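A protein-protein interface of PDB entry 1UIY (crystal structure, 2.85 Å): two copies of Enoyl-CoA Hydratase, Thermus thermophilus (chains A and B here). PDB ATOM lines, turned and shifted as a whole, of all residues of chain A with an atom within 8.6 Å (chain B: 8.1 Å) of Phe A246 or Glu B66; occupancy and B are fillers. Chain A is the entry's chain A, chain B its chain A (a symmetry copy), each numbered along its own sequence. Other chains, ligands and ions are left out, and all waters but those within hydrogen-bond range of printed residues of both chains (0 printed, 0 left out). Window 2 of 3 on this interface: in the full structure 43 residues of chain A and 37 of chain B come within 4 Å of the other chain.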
ATOM      1  N   LEU A 238      17.813   3.803 -33.469  1.00  0.00           N
ATOM      2  CA  LEU A 238      17.106   3.736 -32.199  1.00  0.00           C
ATOM      3  C   LEU A 238      18.056   4.222 -31.122  1.00  0.00           C
ATOM      4  O   LEU A 238      17.662   4.982 -30.230  1.00  0.00           O
ATOM      5  CB  LEU A 238      16.660   2.313 -31.874  1.00  0.00           C
ATOM      6  CG  LEU A 238      15.746   2.250 -30.648  1.00  0.00           C
ATOM      7  CD1 LEU A 238      14.538   3.149 -30.877  1.00  0.00           C
ATOM      8  CD2 LEU A 238      15.307   0.824 -30.385  1.00  0.00           C
ATOM      9  N   ALA A 239      19.310   3.771 -31.208  1.00  0.00           N
ATOM     10  CA  ALA A 239      20.334   4.173 -30.253  1.00  0.00           C
ATOM     11  C   ALA A 239      20.454   5.690 -30.335  1.00  0.00           C
ATOM     12  O   ALA A 239      20.350   6.381 -29.324  1.00  0.00           O
ATOM     13  CB  ALA A 239      21.667   3.516 -30.593  1.00  0.00           C
ATOM     14  N   GLU A 240      20.652   6.199 -31.549  1.00  0.00           N
ATOM     15  CA  GLU A 240      20.771   7.633 -31.769  1.00  0.00           C
ATOM     16  C   GLU A 240      19.587   8.392 -31.193  1.00  0.00           C
ATOM     17  O   GLU A 240      19.754   9.335 -30.432  1.00  0.00           O
ATOM     18  CB  GLU A 240      20.868   7.933 -33.264  1.00  0.00           C
ATOM     19  CG  GLU A 240      20.719   9.404 -33.614  1.00  0.00           C
ATOM     20  CD  GLU A 240      21.646  10.300 -32.812  1.00  0.00           C
ATOM     21  OE1 GLU A 240      22.885  10.155 -32.929  1.00  0.00           O
ATOM     22  OE2 GLU A 240      21.128  11.152 -32.060  1.00  0.00           O
ATOM     23  N   GLY A 241      18.387   7.976 -31.569  1.00  0.00           N
ATOM     24  CA  GLY A 241      17.194   8.642 -31.090  1.00  0.00           C
ATOM     25  C   GLY A 241      17.061   8.686 -29.583  1.00  0.00           C
ATOM     26  O   GLY A 241      16.901   9.760 -29.010  1.00  0.00           O
ATOM     27  N   ILE A 242      17.115   7.525 -28.941  1.00  0.00           N
ATOM     28  CA  ILE A 242      16.985   7.450 -27.492  1.00  0.00           C
ATOM     29  C   ILE A 242      18.021   8.332 -26.788  1.00  0.00           C
ATOM     30  O   ILE A 242      17.750   8.902 -25.731  1.00  0.00           O
ATOM     31  CB  ILE A 242      17.107   5.993 -27.009  1.00  0.00           C
ATOM     32  CG1 ILE A 242      15.936   5.180 -27.566  1.00  0.00           C
ATOM     33  CG2 ILE A 242      17.114   5.940 -25.493  1.00  0.00           C
ATOM     34  CD1 ILE A 242      15.914   3.727 -27.139  1.00  0.00           C
ATOM     35  N   ARG A 243      19.206   8.447 -27.375  1.00  0.00           N
ATOM     36  CA  ARG A 243      20.235   9.293 -26.796  1.00  0.00           C
ATOM     37  C   ARG A 243      19.727  10.727 -26.873  1.00  0.00           C
ATOM     38  O   ARG A 243      19.486  11.371 -25.847  1.00  0.00           O
ATOM     39  CB  ARG A 243      21.545   9.181 -27.578  1.00  0.00           C
ATOM     40  CG  ARG A 243      22.186   7.816 -27.541  1.00  0.00           C
ATOM     41  CD  ARG A 243      23.669   7.934 -27.238  1.00  0.00           C
ATOM     42  NE  ARG A 243      24.391   6.693 -27.502  1.00  0.00           N
ATOM     43  CZ  ARG A 243      24.667   6.235 -28.720  1.00  0.00           C
ATOM     44  NH1 ARG A 243      24.283   6.916 -29.797  1.00  0.00           N
ATOM     45  NH2 ARG A 243      25.331   5.095 -28.863  1.00  0.00           N
ATOM     46  N   ALA A 244      19.563  11.205 -28.105  1.00  0.00           N
ATOM     47  CA  ALA A 244      19.089  12.553 -28.375  1.00  0.00           C
ATOM     48  C   ALA A 244      17.922  12.931 -27.474  1.00  0.00           C
ATOM     49  O   ALA A 244      17.718  14.102 -27.164  1.00  0.00           O
ATOM     50  CB  ALA A 244      18.683  12.672 -29.837  1.00  0.00           C
ATOM     51  N   PHE A 245      17.154  11.937 -27.051  1.00  0.00           N
ATOM     52  CA  PHE A 245      16.022  12.196 -26.179  1.00  0.00           C
ATOM     53  C   PHE A 245      16.526  12.458 -24.770  1.00  0.00           C
ATOM     54  O   PHE A 245      16.047  13.369 -24.093  1.00  0.00           O
ATOM     55  CB  PHE A 245      15.067  11.005 -26.196  1.00  0.00           C
ATOM     56  CG  PHE A 245      13.946  11.113 -25.214  1.00  0.00           C
ATOM     57  CD1 PHE A 245      14.106  10.675 -23.905  1.00  0.00           C
ATOM     58  CD2 PHE A 245      12.717  11.636 -25.600  1.00  0.00           C
ATOM     59  CE1 PHE A 245      13.056  10.751 -22.991  1.00  0.00           C
ATOM     60  CE2 PHE A 245      11.654  11.721 -24.693  1.00  0.00           C
ATOM     61  CZ  PHE A 245      11.825  11.275 -23.385  1.00  0.00           C
ATOM     62  N   PHE A 246      17.498  11.663 -24.334  1.00  0.00           N
ATOM     63  CA  PHE A 246      18.073  11.824 -23.003  1.00  0.00           C
ATOM     64  C   PHE A 246      19.113  12.937 -22.975  1.00  0.00           C
ATOM     65  O   PHE A 246      19.793  13.135 -21.973  1.00  0.00           O
ATOM     66  CB  PHE A 246      18.705  10.514 -22.524  1.00  0.00           C
ATOM     67  CG  PHE A 246      17.709   9.505 -22.024  1.00  0.00           C
ATOM     68  CD1 PHE A 246      16.796   9.846 -21.032  1.00  0.00           C
ATOM     69  CD2 PHE A 246      17.691   8.209 -22.530  1.00  0.00           C
ATOM     70  CE1 PHE A 246      15.883   8.914 -20.552  1.00  0.00           C
ATOM     71  CE2 PHE A 246      16.781   7.268 -22.055  1.00  0.00           C
ATOM     72  CZ  PHE A 246      15.877   7.620 -21.066  1.00  0.00           C
ATOM     73  N   GLU A 247      19.235  13.654 -24.083  1.00  0.00           N
ATOM     74  CA  GLU A 247      20.173  14.764 -24.189  1.00  0.00           C
ATOM     75  C   GLU A 247      19.400  15.973 -24.673  1.00  0.00           C
ATOM     76  O   GLU A 247      19.978  16.945 -25.161  1.00  0.00           O
ATOM     77  CB  GLU A 247      21.285  14.443 -25.179  1.00  0.00           C
ATOM     78  CG  GLU A 247      22.425  13.660 -24.582  1.00  0.00           C
ATOM     79  CD  GLU A 247      23.341  13.098 -25.642  1.00  0.00           C
ATOM     80  OE1 GLU A 247      23.702  13.850 -26.575  1.00  0.00           O
ATOM     81  OE2 GLU A 247      23.697  11.903 -25.537  1.00  0.00           O
ATOM     82  N   LYS A 248      18.081  15.888 -24.549  1.00  0.00           N
ATOM     83  CA  LYS A 248      17.202  16.970 -24.952  1.00  0.00           C
ATOM     84  C   LYS A 248      17.773  17.696 -26.164  1.00  0.00           C
ATOM     85  O   LYS A 248      17.859  18.919 -26.184  1.00  0.00           O
ATOM     86  CB  LYS A 248      17.014  17.916 -23.762  1.00  0.00           C
ATOM     87  CG  LYS A 248      16.550  17.157 -22.519  1.00  0.00           C
ATOM     88  CD  LYS A 248      16.358  18.021 -21.288  1.00  0.00           C
ATOM     89  CE  LYS A 248      15.972  17.145 -20.095  1.00  0.00           C
ATOM     90  NZ  LYS A 248      15.921  17.872 -18.791  1.00  0.00           N
ATOM     91  N   ARG A 249      18.171  16.918 -27.166  1.00  0.00           N
ATOM     92  CA  ARG A 249      18.736  17.455 -28.399  1.00  0.00           C
ATOM     93  C   ARG A 249      18.107  16.776 -29.608  1.00  0.00           C
ATOM     94  O   ARG A 249      17.559  15.677 -29.504  1.00  0.00           O
ATOM     95  CB  ARG A 249      20.247  17.211 -28.450  1.00  0.00           C
ATOM     96  CG  ARG A 249      20.630  15.780 -28.814  1.00  0.00           C
ATOM     97  CD  ARG A 249      22.134  15.613 -28.914  1.00  0.00           C
ATOM     98  NE  ARG A 249      22.531  14.228 -29.178  1.00  0.00           N
ATOM     99  CZ  ARG A 249      22.392  13.608 -30.348  1.00  0.00           C
ATOM    100  NH1 ARG A 249      21.864  14.242 -31.388  1.00  0.00           N
ATOM    101  NH2 ARG A 249      22.791  12.349 -30.482  1.00  0.00           N
ATOM    102  N   PRO A 251      17.710  14.576 -32.903  1.00  0.00           N
ATOM    103  CA  PRO A 251      18.320  13.334 -33.385  1.00  0.00           C
ATOM    104  C   PRO A 251      19.058  13.540 -34.699  1.00  0.00           C
ATOM    105  O   PRO A 251      18.560  14.224 -35.592  1.00  0.00           O
ATOM    106  CB  PRO A 251      17.121  12.412 -33.559  1.00  0.00           C
ATOM    107  CG  PRO A 251      16.171  12.903 -32.524  1.00  0.00           C
ATOM    108  CD  PRO A 251      16.264  14.388 -32.704  1.00  0.00           C
ATOM    109  N   ALA B  60       6.261   7.980 -22.202  1.00  0.00           N
ATOM    110  CA  ALA B  60       7.557   7.343 -22.382  1.00  0.00           C
ATOM    111  C   ALA B  60       8.032   6.659 -21.110  1.00  0.00           C
ATOM    112  O   ALA B  60       8.209   7.303 -20.083  1.00  0.00           O
ATOM    113  CB  ALA B  60       8.588   8.373 -22.830  1.00  0.00           C
ATOM    114  N   ASP B  61       8.225   5.349 -21.178  1.00  0.00           N
ATOM    115  CA  ASP B  61       8.710   4.607 -20.027  1.00  0.00           C
ATOM    116  C   ASP B  61      10.229   4.746 -20.025  1.00  0.00           C
ATOM    117  O   ASP B  61      10.944   3.906 -20.575  1.00  0.00           O
ATOM    118  CB  ASP B  61       8.320   3.133 -20.140  1.00  0.00           C
ATOM    119  CG  ASP B  61       8.738   2.326 -18.927  1.00  0.00           C
ATOM    120  OD1 ASP B  61       9.952   2.269 -18.633  1.00  0.00           O
ATOM    121  OD2 ASP B  61       7.849   1.750 -18.265  1.00  0.00           O
ATOM    122  N   LEU B  62      10.719   5.819 -19.417  1.00  0.00           N
ATOM    123  CA  LEU B  62      12.151   6.077 -19.360  1.00  0.00           C
ATOM    124  C   LEU B  62      12.898   4.873 -18.799  1.00  0.00           C
ATOM    125  O   LEU B  62      14.045   4.608 -19.170  1.00  0.00           O
ATOM    126  CB  LEU B  62      12.419   7.313 -18.501  1.00  0.00           C
ATOM    127  CG  LEU B  62      11.552   8.533 -18.829  1.00  0.00           C
ATOM    128  CD1 LEU B  62      12.076   9.736 -18.062  1.00  0.00           C
ATOM    129  CD2 LEU B  62      11.574   8.805 -20.322  1.00  0.00           C
ATOM    130  N   ALA B  63      12.244   4.149 -17.903  1.00  0.00           N
ATOM    131  CA  ALA B  63      12.845   2.968 -17.306  1.00  0.00           C
ATOM    132  C   ALA B  63      13.153   1.983 -18.419  1.00  0.00           C
ATOM    133  O   ALA B  63      14.126   1.230 -18.358  1.00  0.00           O
ATOM    134  CB  ALA B  63      11.881   2.347 -16.316  1.00  0.00           C
ATOM    135  N   PHE B  64      12.305   2.014 -19.441  1.00  0.00           N
ATOM    136  CA  PHE B  64      12.408   1.142 -20.601  1.00  0.00           C
ATOM    137  C   PHE B  64      13.406   1.647 -21.636  1.00  0.00           C
ATOM    138  O   PHE B  64      14.288   0.901 -22.071  1.00  0.00           O
ATOM    139  CB  PHE B  64      11.026   0.997 -21.242  1.00  0.00           C
ATOM    140  CG  PHE B  64      11.037   0.292 -22.564  1.00  0.00           C
ATOM    141  CD1 PHE B  64      11.457  -1.031 -22.662  1.00  0.00           C
ATOM    142  CD2 PHE B  64      10.625   0.950 -23.715  1.00  0.00           C
ATOM    143  CE1 PHE B  64      11.470  -1.691 -23.886  1.00  0.00           C
ATOM    144  CE2 PHE B  64      10.632   0.301 -24.942  1.00  0.00           C
ATOM    145  CZ  PHE B  64      11.057  -1.026 -25.026  1.00  0.00           C
ATOM    146  N   LEU B  65      13.272   2.909 -22.033  1.00  0.00           N
ATOM    147  CA  LEU B  65      14.172   3.480 -23.027  1.00  0.00           C
ATOM    148  C   LEU B  65      15.630   3.322 -22.621  1.00  0.00           C
ATOM    149  O   LEU B  65      16.503   3.126 -23.467  1.00  0.00           O
ATOM    150  CB  LEU B  65      13.856   4.961 -23.255  1.00  0.00           C
ATOM    151  CG  LEU B  65      12.570   5.280 -24.027  1.00  0.00           C
ATOM    152  CD1 LEU B  65      11.364   4.708 -23.293  1.00  0.00           C
ATOM    153  CD2 LEU B  65      12.427   6.782 -24.199  1.00  0.00           C
ATOM    154  N   GLU B  66      15.893   3.399 -21.323  1.00  0.00           N
ATOM    155  CA  GLU B  66      17.255   3.267 -20.835  1.00  0.00           C
ATOM    156  C   GLU B  66      17.826   1.876 -21.049  1.00  0.00           C
ATOM    157  O   GLU B  66      18.971   1.738 -21.480  1.00  0.00           O
ATOM    158  CB  GLU B  66      17.325   3.628 -19.350  1.00  0.00           C
ATOM    159  CG  GLU B  66      17.431   5.126 -19.085  1.00  0.00           C
ATOM    160  CD  GLU B  66      18.763   5.714 -19.531  1.00  0.00           C
ATOM    161  OE1 GLU B  66      19.059   5.692 -20.744  1.00  0.00           O
ATOM    162  OE2 GLU B  66      19.518   6.199 -18.663  1.00  0.00           O
ATOM    163  N   ARG B  67      17.027   0.853 -20.763  1.00  0.00           N
ATOM    164  CA  ARG B  67      17.475  -0.529 -20.899  1.00  0.00           C
ATOM    165  C   ARG B  67      17.498  -0.995 -22.346  1.00  0.00           C
ATOM    166  O   ARG B  67      18.559  -1.253 -22.913  1.00  0.00           O
ATOM    167  CB  ARG B  67      16.570  -1.468 -20.095  1.00  0.00           C
ATOM    168  CG  ARG B  67      16.242  -0.996 -18.679  1.00  0.00           C
ATOM    169  CD  ARG B  67      17.492  -0.781 -17.831  1.00  0.00           C
ATOM    170  NE  ARG B  67      17.705  -1.838 -16.844  1.00  0.00           N
ATOM    171  CZ  ARG B  67      18.545  -1.730 -15.819  1.00  0.00           C
ATOM    172  NH1 ARG B  67      18.691  -2.734 -14.960  1.00  0.00           N
ATOM    173  NH2 ARG B  67      19.234  -0.607 -15.650  1.00  0.00           N
ATOM    174  N   VAL B  68      16.309  -1.095 -22.928  1.00  0.00           N
ATOM    175  CA  VAL B  68      16.109  -1.553 -24.300  1.00  0.00           C
ATOM    176  C   VAL B  68      17.335  -1.611 -25.212  1.00  0.00           C
ATOM    177  O   VAL B  68      17.697  -2.686 -25.695  1.00  0.00           O
ATOM    178  CB  VAL B  68      15.005  -0.720 -24.987  1.00  0.00           C
ATOM    179  CG1 VAL B  68      15.442   0.724 -25.112  1.00  0.00           C
ATOM    180  CG2 VAL B  68      14.675  -1.312 -26.342  1.00  0.00           C
ATOM    181  N   THR B  69      17.979  -0.474 -25.448  1.00  0.00           N
ATOM    182  CA  THR B  69      19.145  -0.438 -26.331  1.00  0.00           C
ATOM    183  C   THR B  69      20.321  -1.305 -25.912  1.00  0.00           C
ATOM    184  O   THR B  69      21.320  -1.365 -26.624  1.00  0.00           O
ATOM    185  CB  THR B  69      19.685   1.001 -26.523  1.00  0.00           C
ATOM    186  OG1 THR B  69      19.744   1.676 -25.258  1.00  0.00           O
ATOM    187  CG2 THR B  69      18.808   1.774 -27.494  1.00  0.00           C
ATOM    188  N   GLU B  70      20.210  -1.976 -24.770  1.00  0.00           N
ATOM    189  CA  GLU B  70      21.300  -2.821 -24.295  1.00  0.00           C
ATOM    190  C   GLU B  70      20.918  -4.288 -24.115  1.00  0.00           C
ATOM    191  O   GLU B  70      21.785  -5.125 -23.870  1.00  0.00           O
ATOM    192  CB  GLU B  70      21.850  -2.279 -22.975  1.00  0.00           C
ATOM    193  CG  GLU B  70      22.442  -0.887 -23.062  1.00  0.00           C
ATOM    194  CD  GLU B  70      21.718   0.098 -22.165  1.00  0.00           C
ATOM    195  OE1 GLU B  70      21.663  -0.146 -20.939  1.00  0.00           O
ATOM    196  OE2 GLU B  70      21.202   1.115 -22.688  1.00  0.00           O
ATOM    197  N   LEU B  71      19.631  -4.598 -24.227  1.00  0.00           N
ATOM    198  CA  LEU B  71      19.172  -5.974 -24.074  1.00  0.00           C
ATOM    199  C   LEU B  71      19.706  -6.837 -25.206  1.00  0.00           C
ATOM    200  O   LEU B  71      20.121  -6.323 -26.250  1.00  0.00           O
ATOM    201  CB  LEU B  71      17.646  -6.034 -24.069  1.00  0.00           C
ATOM    202  CG  LEU B  71      16.928  -5.417 -22.871  1.00  0.00           C
ATOM    203  CD1 LEU B  71      15.423  -5.539 -23.049  1.00  0.00           C
ATOM    204  CD2 LEU B  71      17.366  -6.127 -21.610  1.00  0.00           C
ATOM    205  N   ILE B 134      11.397   8.579 -33.123  1.00  0.00           N
ATOM    206  CA  ILE B 134      12.545   8.281 -32.284  1.00  0.00           C
ATOM    207  C   ILE B 134      13.349   7.059 -32.701  1.00  0.00           C
ATOM    208  O   ILE B 134      14.405   6.790 -32.134  1.00  0.00           O
ATOM    209  CB  ILE B 134      12.115   8.126 -30.802  1.00  0.00           C
ATOM    210  CG1 ILE B 134      13.340   8.208 -29.884  1.00  0.00           C
ATOM    211  CG2 ILE B 134      11.401   6.799 -30.596  1.00  0.00           C
ATOM    212  CD1 ILE B 134      12.994   8.310 -28.410  1.00  0.00           C
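The side-chain carboxylate (OE2) of Glu B70 is in hydrogen-bond range of the side-chain hydroxyl (OG1) of Thr B69 (3.0 Å). O of Glu B66 lies close to OE2 of Glu B70 (2.6 Å).
No position is printed for both chains. Of the 10 pairs that touch across the chains among the printed residues, none has its exchanged pair printed and touching as well.
Of the printed residues of chain B, Phe A246 touches Leu B65 (3.9 Å) and Glu B66 (3.1 Å). Glu B66 touches one residue of chain A. Printed residues of chain A within 4 Å of Thr B69: Ala A239 and Ile A242. Of the printed residues of chain B, Ala A239 touches Thr B69 (3.96 Å). Of the printed residues of chain A, Leu B62 touches Phe A245 (3.6 Å). Of the printed residues of chain A, Val B68 touches Ile A242 (3.7 Å). Asp B61 touches none of the printed residues of chain A. Glu A247 touches none of the printed residues of chain B. The nearest printed residue of chain A that does not touch Ile B134 is Phe A245 (4.1 Å).
Printed residues of chain A that touch a printed residue of chain B: Leu A238, Ala A239, Gly A241, Ile A242, Phe A245 and Phe A246. Hydrophobic or aromatic side chains of chain A within 4 Å of the printed part of chain B: Leu A238, Ile A242, Phe A245 and Phe A246. Printed residues of chain B that touch a printed residue of chain A: Leu B62, Leu B65, Glu B66, Val B68, Thr B69 and Ile B134. Hydrophobic or aromatic side chains of chain B within 4 Å of the printed part of chain A: Leu B62, Leu B65, Val B68 and Ile B134. Among the printed residues, 10 pairs touch across the chains. Among the printed residues, no Asp or Glu carboxylate lies within 4 Å of a Lys or Arg side-chain nitrogen of the other chain.
O of Ile B134 touches CD1 of Leu A238, 3.9 Å away. Ala A239 touches Thr B69 (CA to CG2, 3.96 Å). Gly A241 touches Ile B134 (CA to O, 3.5 Å). Leu B65 touches Ile A242. CG1 of Val B68 touches CD1 of Ile A242 (3.7 Å). Ile A242 touches Thr B69 (CD1 to CG2, 3.5 Å). Ile B134 touches Ile A242. Leu B62 touches Phe A245 (CD2 to CE1, 3.6 Å). Phe A246 touches Leu B65. Phe A246 touches Glu B66 (CE2 to OE1, 3.1 Å).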
